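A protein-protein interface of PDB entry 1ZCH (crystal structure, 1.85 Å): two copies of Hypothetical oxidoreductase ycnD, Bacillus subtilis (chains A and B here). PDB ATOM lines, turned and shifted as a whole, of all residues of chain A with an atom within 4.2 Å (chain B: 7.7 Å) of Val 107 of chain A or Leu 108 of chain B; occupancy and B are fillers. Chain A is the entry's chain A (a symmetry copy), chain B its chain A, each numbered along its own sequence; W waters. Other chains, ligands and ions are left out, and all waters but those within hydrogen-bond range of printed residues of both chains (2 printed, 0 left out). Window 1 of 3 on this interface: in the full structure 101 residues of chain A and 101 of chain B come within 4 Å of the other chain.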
ATOM      1  N   LEU A 104     -11.701 -22.222  14.844  1.00  0.00           N
ATOM      2  CA  LEU A 104     -10.251 -22.289  15.007  1.00  0.00           C
ATOM      3  C   LEU A 104      -9.712 -21.714  16.316  1.00  0.00           C
ATOM      4  O   LEU A 104      -8.560 -21.960  16.673  1.00  0.00           O
ATOM      5  CB  LEU A 104      -9.557 -21.618  13.815  1.00  0.00           C
ATOM      6  CG  LEU A 104      -9.652 -22.425  12.510  1.00  0.00           C
ATOM      7  CD1 LEU A 104      -9.062 -21.637  11.350  1.00  0.00           C
ATOM      8  CD2 LEU A 104      -8.917 -23.749  12.685  1.00  0.00           C
ATOM      9  N   GLU A 105     -10.531 -20.960  17.042  1.00  0.00           N
ATOM     10  CA  GLU A 105     -10.082 -20.401  18.316  1.00  0.00           C
ATOM     11  C   GLU A 105      -9.612 -21.536  19.230  1.00  0.00           C
ATOM     12  O   GLU A 105      -8.618 -21.397  19.944  1.00  0.00           O
ATOM     13  CB  GLU A 105     -11.217 -19.615  18.986  1.00  0.00           C
ATOM     14  CG  GLU A 105     -10.980 -19.234  20.455  1.00  0.00           C
ATOM     15  CD  GLU A 105      -9.759 -18.343  20.680  1.00  0.00           C
ATOM     16  OE1 GLU A 105      -9.202 -17.798  19.702  1.00  0.00           O
ATOM     17  OE2 GLU A 105      -9.362 -18.176  21.856  1.00  0.00           O
ATOM     18  N   SER A 106     -10.326 -22.661  19.199  1.00  0.00           N
ATOM     19  CA  SER A 106      -9.969 -23.814  20.026  1.00  0.00           C
ATOM     20  C   SER A 106      -8.597 -24.350  19.625  1.00  0.00           C
ATOM     21  O   SER A 106      -7.800 -24.746  20.476  1.00  0.00           O
ATOM     22  CB  SER A 106     -11.017 -24.924  19.879  1.00  0.00           C
ATOM     23  OG  SER A 106     -11.140 -25.333  18.527  1.00  0.00           O
ATOM     24  N   VAL A 107      -8.328 -24.354  18.323  1.00  0.00           N
ATOM     25  CA  VAL A 107      -7.052 -24.835  17.808  1.00  0.00           C
ATOM     26  C   VAL A 107      -5.923 -23.926  18.294  1.00  0.00           C
ATOM     27  O   VAL A 107      -4.860 -24.406  18.695  1.00  0.00           O
ATOM     28  CB  VAL A 107      -7.065 -24.887  16.256  1.00  0.00           C
ATOM     29  CG1 VAL A 107      -5.663 -25.178  15.717  1.00  0.00           C
ATOM     30  CG2 VAL A 107      -8.048 -25.968  15.787  1.00  0.00           C
ATOM     31  N   LEU A 108      -6.150 -22.617  18.270  1.00  0.00           N
ATOM     32  CA  LEU A 108      -5.126 -21.689  18.732  1.00  0.00           C
ATOM     33  C   LEU A 108      -4.915 -21.867  20.231  1.00  0.00           C
ATOM     34  O   LEU A 108      -3.780 -21.876  20.705  1.00  0.00           O
ATOM     35  CB  LEU A 108      -5.520 -20.237  18.432  1.00  0.00           C
ATOM     36  CG  LEU A 108      -5.641 -19.853  16.953  1.00  0.00           C
ATOM     37  CD1 LEU A 108      -5.940 -18.364  16.845  1.00  0.00           C
ATOM     38  CD2 LEU A 108      -4.352 -20.200  16.210  1.00  0.00           C
ATOM     39  N   VAL A 109      -6.005 -22.007  20.981  1.00  0.00           N
ATOM     40  CA  VAL A 109      -5.889 -22.196  22.430  1.00  0.00           C
ATOM     41  C   VAL A 109      -5.050 -23.437  22.738  1.00  0.00           C
ATOM     42  O   VAL A 109      -4.129 -23.392  23.555  1.00  0.00           O
ATOM     43  CB  VAL A 109      -7.281 -22.354  23.101  1.00  0.00           C
ATOM     44  CG1 VAL A 109      -7.118 -22.810  24.553  1.00  0.00           C
ATOM     45  CG2 VAL A 109      -8.028 -21.027  23.056  1.00  0.00           C
ATOM     46  N   GLY A 110      -5.373 -24.541  22.073  1.00  0.00           N
ATOM     47  CA  GLY A 110      -4.645 -25.776  22.299  1.00  0.00           C
ATOM     48  C   GLY A 110      -3.183 -25.727  21.889  1.00  0.00           C
ATOM     49  O   GLY A 110      -2.313 -26.223  22.614  1.00  0.00           O
ATOM     50  N   ALA A 111      -2.909 -25.133  20.731  1.00  0.00           N
ATOM     51  CA  ALA A 111      -1.541 -25.038  20.225  1.00  0.00           C
ATOM     52  C   ALA A 111      -0.676 -24.147  21.112  1.00  0.00           C
ATOM     53  O   ALA A 111       0.485 -24.463  21.376  1.00  0.00           O
ATOM     54  CB  ALA A 111      -1.547 -24.509  18.786  1.00  0.00           C
ATOM     55  N   ARG A 139       3.298 -34.694  13.411  1.00  0.00           N
ATOM     56  CA  ARG A 139       2.145 -34.256  12.639  1.00  0.00           C
ATOM     57  C   ARG A 139       2.164 -34.811  11.210  1.00  0.00           C
ATOM     58  O   ARG A 139       1.254 -34.541  10.427  1.00  0.00           O
ATOM     59  CB  ARG A 139       2.074 -32.722  12.601  1.00  0.00           C
ATOM     60  CG  ARG A 139       1.927 -32.071  13.977  1.00  0.00           C
ATOM     61  CD  ARG A 139       1.239 -30.709  13.886  1.00  0.00           C
ATOM     62  NE  ARG A 139       2.052 -29.681  13.240  1.00  0.00           N
ATOM     63  CZ  ARG A 139       2.887 -28.866  13.880  1.00  0.00           C
ATOM     64  NH1 ARG A 139       3.030 -28.956  15.197  1.00  0.00           N
ATOM     65  NH2 ARG A 139       3.565 -27.942  13.208  1.00  0.00           N
ATOM     66  N   LEU A 158       0.711 -32.413  18.671  1.00  0.00           N
ATOM     67  CA  LEU A 158       1.327 -31.184  18.191  1.00  0.00           C
ATOM     68  C   LEU A 158       2.837 -31.342  18.075  1.00  0.00           C
ATOM     69  O   LEU A 158       3.421 -31.035  17.038  1.00  0.00           O
ATOM     70  CB  LEU A 158       0.977 -30.019  19.119  1.00  0.00           C
ATOM     71  CG  LEU A 158      -0.447 -29.515  18.873  1.00  0.00           C
ATOM     72  CD1 LEU A 158      -0.893 -28.596  19.988  1.00  0.00           C
ATOM     73  CD2 LEU A 158      -0.483 -28.799  17.525  1.00  0.00           C
ATOM     74  N   ILE A 236      -3.430 -31.405   7.494  1.00  0.00           N
ATOM     75  CA  ILE A 236      -3.729 -30.902   8.832  1.00  0.00           C
ATOM     76  C   ILE A 236      -5.206 -30.635   9.098  1.00  0.00           C
ATOM     77  O   ILE A 236      -5.736 -31.060  10.127  1.00  0.00           O
ATOM     78  CB  ILE A 236      -2.917 -29.622   9.150  1.00  0.00           C
ATOM     79  CG1 ILE A 236      -1.422 -29.950   9.154  1.00  0.00           C
ATOM     80  CG2 ILE A 236      -3.328 -29.062  10.517  1.00  0.00           C
ATOM     81  CD1 ILE A 236      -1.033 -31.053  10.134  1.00  0.00           C
ATOM     82  N   PHE A 245     -12.510 -31.178  15.608  1.00  0.00           N
ATOM     83  CA  PHE A 245     -12.312 -29.740  15.490  1.00  0.00           C
ATOM     84  C   PHE A 245     -12.836 -29.282  14.136  1.00  0.00           C
ATOM     85  O   PHE A 245     -12.454 -29.824  13.097  1.00  0.00           O
ATOM     86  CB  PHE A 245     -10.828 -29.399  15.623  1.00  0.00           C
ATOM     87  CG  PHE A 245     -10.278 -29.635  17.000  1.00  0.00           C
ATOM     88  CD1 PHE A 245     -10.338 -28.636  17.968  1.00  0.00           C
ATOM     89  CD2 PHE A 245      -9.727 -30.867  17.340  1.00  0.00           C
ATOM     90  CE1 PHE A 245      -9.857 -28.859  19.255  1.00  0.00           C
ATOM     91  CE2 PHE A 245      -9.242 -31.101  18.630  1.00  0.00           C
ATOM     92  CZ  PHE A 245      -9.308 -30.095  19.587  1.00  0.00           C
ATOM     93  N   SER B  40      10.529 -24.456  15.333  1.00  0.00           N
ATOM     94  CA  SER B  40      10.462 -25.392  14.213  1.00  0.00           C
ATOM     95  C   SER B  40      11.420 -24.973  13.092  1.00  0.00           C
ATOM     96  O   SER B  40      11.365 -23.833  12.613  1.00  0.00           O
ATOM     97  CB  SER B  40       9.024 -25.474  13.698  1.00  0.00           C
ATOM     98  OG  SER B  40       8.871 -26.548  12.789  1.00  0.00           O
ATOM     99  N   ALA B  81       2.488 -14.792  15.757  1.00  0.00           N
ATOM    100  CA  ALA B  81       3.000 -15.836  14.880  1.00  0.00           C
ATOM    101  C   ALA B  81       3.537 -14.974  13.737  1.00  0.00           C
ATOM    102  O   ALA B  81       2.898 -13.986  13.361  1.00  0.00           O
ATOM    103  CB  ALA B  81       1.864 -16.723  14.391  1.00  0.00           C
ATOM    104  N   PHE B  83       5.216 -15.182   9.788  1.00  0.00           N
ATOM    105  CA  PHE B  83       5.690 -15.851   8.580  1.00  0.00           C
ATOM    106  C   PHE B  83       6.050 -14.767   7.562  1.00  0.00           C
ATOM    107  O   PHE B  83       6.202 -15.036   6.367  1.00  0.00           O
ATOM    108  CB  PHE B  83       4.621 -16.803   8.024  1.00  0.00           C
ATOM    109  CG  PHE B  83       4.663 -18.178   8.637  1.00  0.00           C
ATOM    110  CD1 PHE B  83       5.427 -19.187   8.062  1.00  0.00           C
ATOM    111  CD2 PHE B  83       3.975 -18.449   9.819  1.00  0.00           C
ATOM    112  CE1 PHE B  83       5.511 -20.455   8.655  1.00  0.00           C
ATOM    113  CE2 PHE B  83       4.051 -19.709  10.421  1.00  0.00           C
ATOM    114  CZ  PHE B  83       4.820 -20.712   9.838  1.00  0.00           C
ATOM    115  N   GLY B 103      -1.977 -23.632   4.204  1.00  0.00           N
ATOM    116  CA  GLY B 103      -2.534 -24.756   4.935  1.00  0.00           C
ATOM    117  C   GLY B 103      -2.394 -24.487   6.421  1.00  0.00           C
ATOM    118  O   GLY B 103      -1.531 -23.708   6.826  1.00  0.00           O
ATOM    119  N   LEU B 104      -3.232 -25.120   7.237  1.00  0.00           N
ATOM    120  CA  LEU B 104      -3.190 -24.914   8.683  1.00  0.00           C
ATOM    121  C   LEU B 104      -1.883 -25.317   9.363  1.00  0.00           C
ATOM    122  O   LEU B 104      -1.640 -24.941  10.509  1.00  0.00           O
ATOM    123  CB  LEU B 104      -4.371 -25.630   9.350  1.00  0.00           C
ATOM    124  CG  LEU B 104      -5.729 -24.959   9.089  1.00  0.00           C
ATOM    125  CD1 LEU B 104      -6.859 -25.797   9.666  1.00  0.00           C
ATOM    126  CD2 LEU B 104      -5.727 -23.566   9.709  1.00  0.00           C
ATOM    127  N   GLU B 105      -1.032 -26.068   8.671  1.00  0.00           N
ATOM    128  CA  GLU B 105       0.246 -26.466   9.258  1.00  0.00           C
ATOM    129  C   GLU B 105       1.019 -25.214   9.684  1.00  0.00           C
ATOM    130  O   GLU B 105       1.662 -25.201  10.734  1.00  0.00           O
ATOM    131  CB  GLU B 105       1.068 -27.281   8.251  1.00  0.00           C
ATOM    132  CG  GLU B 105       2.541 -27.502   8.625  1.00  0.00           C
ATOM    133  CD  GLU B 105       2.745 -28.261   9.936  1.00  0.00           C
ATOM    134  OE1 GLU B 105       1.777 -28.843  10.471  1.00  0.00           O
ATOM    135  OE2 GLU B 105       3.896 -28.283  10.429  1.00  0.00           O
ATOM    136  N   SER B 106       0.947 -24.163   8.869  1.00  0.00           N
ATOM    137  CA  SER B 106       1.641 -22.912   9.174  1.00  0.00           C
ATOM    138  C   SER B 106       1.089 -22.299  10.459  1.00  0.00           C
ATOM    139  O   SER B 106       1.839 -21.759  11.274  1.00  0.00           O
ATOM    140  CB  SER B 106       1.482 -21.915   8.020  1.00  0.00           C
ATOM    141  OG  SER B 106       0.114 -21.645   7.765  1.00  0.00           O
ATOM    142  N   VAL B 107      -0.225 -22.393  10.634  1.00  0.00           N
ATOM    143  CA  VAL B 107      -0.878 -21.854  11.820  1.00  0.00           C
ATOM    144  C   VAL B 107      -0.405 -22.613  13.061  1.00  0.00           C
ATOM    145  O   VAL B 107      -0.132 -22.008  14.100  1.00  0.00           O
ATOM    146  CB  VAL B 107      -2.423 -21.947  11.694  1.00  0.00           C
ATOM    147  CG1 VAL B 107      -3.093 -21.587  13.022  1.00  0.00           C
ATOM    148  CG2 VAL B 107      -2.905 -21.002  10.585  1.00  0.00           C
ATOM    149  N   LEU B 108      -0.299 -23.933  12.955  1.00  0.00           N
ATOM    150  CA  LEU B 108       0.160 -24.723  14.090  1.00  0.00           C
ATOM    151  C   LEU B 108       1.616 -24.389  14.389  1.00  0.00           C
ATOM    152  O   LEU B 108       1.997 -24.239  15.549  1.00  0.00           O
ATOM    153  CB  LEU B 108       0.017 -26.226  13.813  1.00  0.00           C
ATOM    154  CG  LEU B 108      -1.409 -26.753  13.624  1.00  0.00           C
ATOM    155  CD1 LEU B 108      -1.365 -28.266  13.457  1.00  0.00           C
ATOM    156  CD2 LEU B 108      -2.278 -26.367  14.819  1.00  0.00           C
ATOM    157  N   VAL B 109       2.435 -24.275  13.346  1.00  0.00           N
ATOM    158  CA  VAL B 109       3.848 -23.943  13.546  1.00  0.00           C
ATOM    159  C   VAL B 109       3.982 -22.611  14.286  1.00  0.00           C
ATOM    160  O   VAL B 109       4.725 -22.501  15.263  1.00  0.00           O
ATOM    161  CB  VAL B 109       4.610 -23.844  12.196  1.00  0.00           C
ATOM    162  CG1 VAL B 109       6.000 -23.243  12.418  1.00  0.00           C
ATOM    163  CG2 VAL B 109       4.739 -25.229  11.574  1.00  0.00           C
ATOM    164  N   GLY B 110       3.252 -21.605  13.816  1.00  0.00           N
ATOM    165  CA  GLY B 110       3.313 -20.296  14.441  1.00  0.00           C
ATOM    166  C   GLY B 110       2.796 -20.258  15.868  1.00  0.00           C
ATOM    167  O   GLY B 110       3.405 -19.624  16.737  1.00  0.00           O
ATOM    168  N   ALA B 111       1.674 -20.930  16.114  1.00  0.00           N
ATOM    169  CA  ALA B 111       1.073 -20.954  17.446  1.00  0.00           C
ATOM    170  C   ALA B 111       1.963 -21.682  18.450  1.00  0.00           C
ATOM    171  O   ALA B 111       2.107 -21.243  19.592  1.00  0.00           O
ATOM    172  CB  ALA B 111      -0.310 -21.613  17.387  1.00  0.00           C
ATOM    173  N   VAL B 112       2.558 -22.796  18.031  1.00  0.00           N
ATOM    174  CA  VAL B 112       3.436 -23.544  18.928  1.00  0.00           C
ATOM    175  C   VAL B 112       4.715 -22.752  19.204  1.00  0.00           C
ATOM    176  O   VAL B 112       5.181 -22.699  20.343  1.00  0.00           O
ATOM    177  CB  VAL B 112       3.796 -24.934  18.343  1.00  0.00           C
ATOM    178  CG1 VAL B 112       4.855 -25.626  19.216  1.00  0.00           C
ATOM    179  CG2 VAL B 112       2.541 -25.792  18.264  1.00  0.00           C
ATOM    180  N   ASP B 113       5.287 -22.139  18.170  1.00  0.00           N
ATOM    181  CA  ASP B 113       6.500 -21.347  18.361  1.00  0.00           C
ATOM    182  C   ASP B 113       6.188 -20.205  19.338  1.00  0.00           C
ATOM    183  O   ASP B 113       6.977 -19.916  20.237  1.00  0.00           O
ATOM    184  CB  ASP B 113       6.994 -20.771  17.021  1.00  0.00           C
ATOM    185  CG  ASP B 113       8.027 -21.667  16.317  1.00  0.00           C
ATOM    186  OD1 ASP B 113       8.199 -22.849  16.692  1.00  0.00           O
ATOM    187  OD2 ASP B 113       8.672 -21.182  15.361  1.00  0.00           O
ATOM    188  N   ALA B 114       5.033 -19.567  19.162  1.00  0.00           N
ATOM    189  CA  ALA B 114       4.631 -18.463  20.034  1.00  0.00           C
ATOM    190  C   ALA B 114       4.393 -18.920  21.475  1.00  0.00           C
ATOM    191  O   ALA B 114       4.705 -18.197  22.421  1.00  0.00           O
ATOM    192  CB  ALA B 114       3.377 -17.789  19.482  1.00  0.00           C
ATOM    193  N   GLY B 115       3.829 -20.116  21.636  1.00  0.00           N
ATOM    194  CA  GLY B 115       3.586 -20.644  22.971  1.00  0.00           C
ATOM    195  C   GLY B 115       4.910 -20.923  23.664  1.00  0.00           C
ATOM    196  O   GLY B 115       5.083 -20.663  24.862  1.00  0.00           O
ATOM    197  N   ARG B 139      -6.904 -11.591  20.877  1.00  0.00           N
ATOM    198  CA  ARG B 139      -7.544 -12.196  19.719  1.00  0.00           C
ATOM    199  C   ARG B 139      -9.012 -11.776  19.585  1.00  0.00           C
ATOM    200  O   ARG B 139      -9.694 -12.195  18.651  1.00  0.00           O
ATOM    201  CB  ARG B 139      -7.444 -13.728  19.787  1.00  0.00           C
ATOM    202  CG  ARG B 139      -6.009 -14.258  19.798  1.00  0.00           C
ATOM    203  CD  ARG B 139      -5.928 -15.677  19.235  1.00  0.00           C
ATOM    204  NE  ARG B 139      -6.546 -16.687  20.092  1.00  0.00           N
ATOM    205  CZ  ARG B 139      -5.905 -17.364  21.042  1.00  0.00           C
ATOM    206  NH1 ARG B 139      -4.616 -17.140  21.269  1.00  0.00           N
ATOM    207  NH2 ARG B 139      -6.547 -18.285  21.754  1.00  0.00           N
ATOM    208  N   PHE B 156       0.136 -12.521  12.816  1.00  0.00           N
ATOM    209  CA  PHE B 156      -1.117 -12.416  13.556  1.00  0.00           C
ATOM    210  C   PHE B 156      -0.895 -12.550  15.057  1.00  0.00           C
ATOM    211  O   PHE B 156      -0.059 -13.335  15.514  1.00  0.00           O
ATOM    212  CB  PHE B 156      -2.164 -13.422  13.036  1.00  0.00           C
ATOM    213  CG  PHE B 156      -1.826 -14.867  13.268  1.00  0.00           C
ATOM    214  CD1 PHE B 156      -2.110 -15.478  14.485  1.00  0.00           C
ATOM    215  CD2 PHE B 156      -1.280 -15.637  12.244  1.00  0.00           C
ATOM    216  CE1 PHE B 156      -1.862 -16.842  14.676  1.00  0.00           C
ATOM    217  CE2 PHE B 156      -1.026 -16.999  12.424  1.00  0.00           C
ATOM    218  CZ  PHE B 156      -1.319 -17.603  13.643  1.00  0.00           C
ATOM    219  N   LEU B 158      -1.281 -13.589  18.889  1.00  0.00           N
ATOM    220  CA  LEU B 158      -1.701 -14.800  19.582  1.00  0.00           C
ATOM    221  C   LEU B 158      -1.948 -14.523  21.058  1.00  0.00           C
ATOM    222  O   LEU B 158      -2.997 -14.874  21.593  1.00  0.00           O
ATOM    223  CB  LEU B 158      -0.652 -15.899  19.407  1.00  0.00           C
ATOM    224  CG  LEU B 158      -0.740 -16.545  18.023  1.00  0.00           C
ATOM    225  CD1 LEU B 158       0.481 -17.391  17.743  1.00  0.00           C
ATOM    226  CD2 LEU B 158      -2.015 -17.383  17.958  1.00  0.00           C
ATOM    227  N   ILE B 236     -11.971 -15.981  14.083  1.00  0.00           N
ATOM    228  CA  ILE B 236     -10.575 -16.381  13.927  1.00  0.00           C
ATOM    229  C   ILE B 236     -10.172 -16.749  12.503  1.00  0.00           C
ATOM    230  O   ILE B 236      -9.145 -16.278  12.010  1.00  0.00           O
ATOM    231  CB  ILE B 236     -10.213 -17.552  14.874  1.00  0.00           C
ATOM    232  CG1 ILE B 236     -10.354 -17.098  16.329  1.00  0.00           C
ATOM    233  CG2 ILE B 236      -8.774 -18.016  14.615  1.00  0.00           C
ATOM    234  CD1 ILE B 236      -9.506 -15.879  16.682  1.00  0.00           C
ATOM    235  N   LEU B 240      -7.235 -14.874  10.245  1.00  0.00           N
ATOM    236  CA  LEU B 240      -6.154 -15.623   9.619  1.00  0.00           C
ATOM    237  C   LEU B 240      -6.105 -15.422   8.108  1.00  0.00           C
ATOM    238  O   LEU B 240      -5.038 -15.168   7.547  1.00  0.00           O
ATOM    239  CB  LEU B 240      -6.295 -17.111   9.952  1.00  0.00           C
ATOM    240  CG  LEU B 240      -6.086 -17.444  11.436  1.00  0.00           C
ATOM    241  CD1 LEU B 240      -6.465 -18.897  11.717  1.00  0.00           C
ATOM    242  CD2 LEU B 240      -4.627 -17.183  11.806  1.00  0.00           C
ATOM    243  N   PHE B 245      -3.180 -16.235   5.657  1.00  0.00           N
ATOM    244  CA  PHE B 245      -3.190 -17.655   5.979  1.00  0.00           C
ATOM    245  C   PHE B 245      -4.453 -18.280   5.405  1.00  0.00           C
ATOM    246  O   PHE B 245      -5.562 -17.806   5.662  1.00  0.00           O
ATOM    247  CB  PHE B 245      -3.145 -17.853   7.493  1.00  0.00           C
ATOM    248  CG  PHE B 245      -1.840 -17.444   8.115  1.00  0.00           C
ATOM    249  CD1 PHE B 245      -0.788 -18.351   8.216  1.00  0.00           C
ATOM    250  CD2 PHE B 245      -1.652 -16.143   8.572  1.00  0.00           C
ATOM    251  CE1 PHE B 245       0.434 -17.969   8.764  1.00  0.00           C
ATOM    252  CE2 PHE B 245      -0.429 -15.750   9.123  1.00  0.00           C
ATOM    253  CZ  PHE B 245       0.614 -16.665   9.218  1.00  0.00           C
HETATM  254  O   HOH W   1       5.589 -29.857  11.980  1.00  0.00           O
HETATM  255  O   HOH W   2      -8.090 -16.324  23.500  1.00  0.00           O
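Of the 12 printed residues of chain A, 8 touch a printed residue of chain B.
Hydrophobic or aromatic side chains of chain A that line the printed part of chain B: Leu 104, Val 107, Leu 108, Val 109, Ala 111 and Ile 236.
Of the 22 printed residues of chain B, 10 touch a printed residue of chain A.
Printed residues of chain B that touch a printed residue of chain A: Leu 104, Glu 105, Val 107, Leu 108, Val 109, Ala 111, Val 112, Arg 139, Ile 236 and Leu 240.
Hydrophobic or aromatic side chains of chain B that line the printed part of chain A: Leu 104, Val 107, Leu 108, Val 109, Ala 111, Val 112, Ile 236 and Leu 240.
Among the printed residues, Asp or Glu carboxylates within 4 Å of a Lys or Arg side-chain nitrogen of the other chain: Glu 105 of chain A with Arg 139 of chain B (2.8 Å) and Arg 139 of chain A with Glu 105 of chain B (2.8 Å).
Leu 104 of chain A touches Ile 236 of chain B, and with the chains exchanged Ile 236 of chain A touches Leu 104 of chain B.
Glu 105 of chain A touches Ile 236 of chain B, and with the chains exchanged Ile 236 of chain A touches Glu 105 of chain B.
Leu 108 of chain A touches Arg 139 of chain B, and with the chains exchanged Arg 139 of chain A touches Leu 108 of chain B.
Ala 111 of chain A touches its own counterpart, Ala 111 of chain B.
Positions printed for both chains: 104, 105, 106, 107, 108, 109, 110, 111, 139, 158, 236 and 245.
NH2 of Arg 139 of chain A is in salt-bridge range of OE2 of Glu 105 of chain B.
The guanidinium group of Arg 139 of chain B lies within salt-bridge range of the side-chain carboxylate of Glu 105 of chain A (2.8 Å).
Water W1 lies within hydrogen-bond range of the side-chain carboxylate of Glu 105 of chain B (2.8 Å) and the guanidinium group of Arg 139 of chain A (3.0 Å).
Water W2 lies within hydrogen-bond range of OE2 of Glu 105 of chain A (2.8 Å) and NH2 of Arg 139 of chain B (3.0 Å).
NH1 of Arg 139 of chain A is in hydrogen-bond range of O of Leu 158 of chain A (2.8 Å).
O of Leu 240 of chain B lies within hydrogen-bond range of N of Phe 245 of chain B (2.9 Å).
NH1 of Arg 139 of chain B sits at hydrogen-bond distance from O of Leu 158 of chain B (2.8 Å).
Printed residues of chain B within 4 Å of Leu 104 of chain A: Ile 236 (3.8 Å) and Leu 240 (3.8 Å).
Printed residues of chain B within 4 Å of Glu 105 of chain A: Arg 139 (2.8 Å) and Ile 236 (3.6 Å).
Printed residues of chain B within 4 Å of Val 107 of chain A: Leu 108 (3.7 Å).
Printed residues of chain B within 4 Å of Val 109 of chain A: Arg 139.
Gly 110 of chain A touches none of the printed residues of chain B.
Leu 108 of chain B touches three residues of chain A.
Printed residues of chain A within 4 Å of Ala 111 of chain B: Ala 111.
Gly 115 of chain B touches none of the printed residues of chain A.
Printed residues of chain A within 4 Å of Leu 240 of chain B: Leu 104.
The nearest residue of chain B that does not touch Val 107 of chain A is Val 107 of chain B (5.2 Å).
The nearest printed residue of chain B that does not touch Leu 108 of chain A is Leu 158 of chain B (4.1 Å).
CB of Leu 104 of chain A touches CG2 of Ile 236 of chain B, 3.8 Å away.
Glu 105 of chain A touches Ile 236 of chain B (OE1 to CD1, 3.6 Å).
Val 107 of chain A touches Leu 108 of chain B.
Val 107 of chain B touches Leu 108 of chain A.
Leu 108 of chain A touches Arg 139 of chain B.
Val 109 of chain A touches Arg 139 of chain B (CG2 to NH2, 3.4 Å).
CB of Ala 111 of chain A touches CB of Ala 111 of chain B, 3.4 Å away.
CD of Arg 139 of chain A touches CD1 of Leu 108 of chain B, 3.6 Å away.
Ile 236 of chain A touches Glu 105 of chain B.
CD1 of Leu 108 of chain B touches CG2 of Ile 236 of chain A (3.6 Å).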
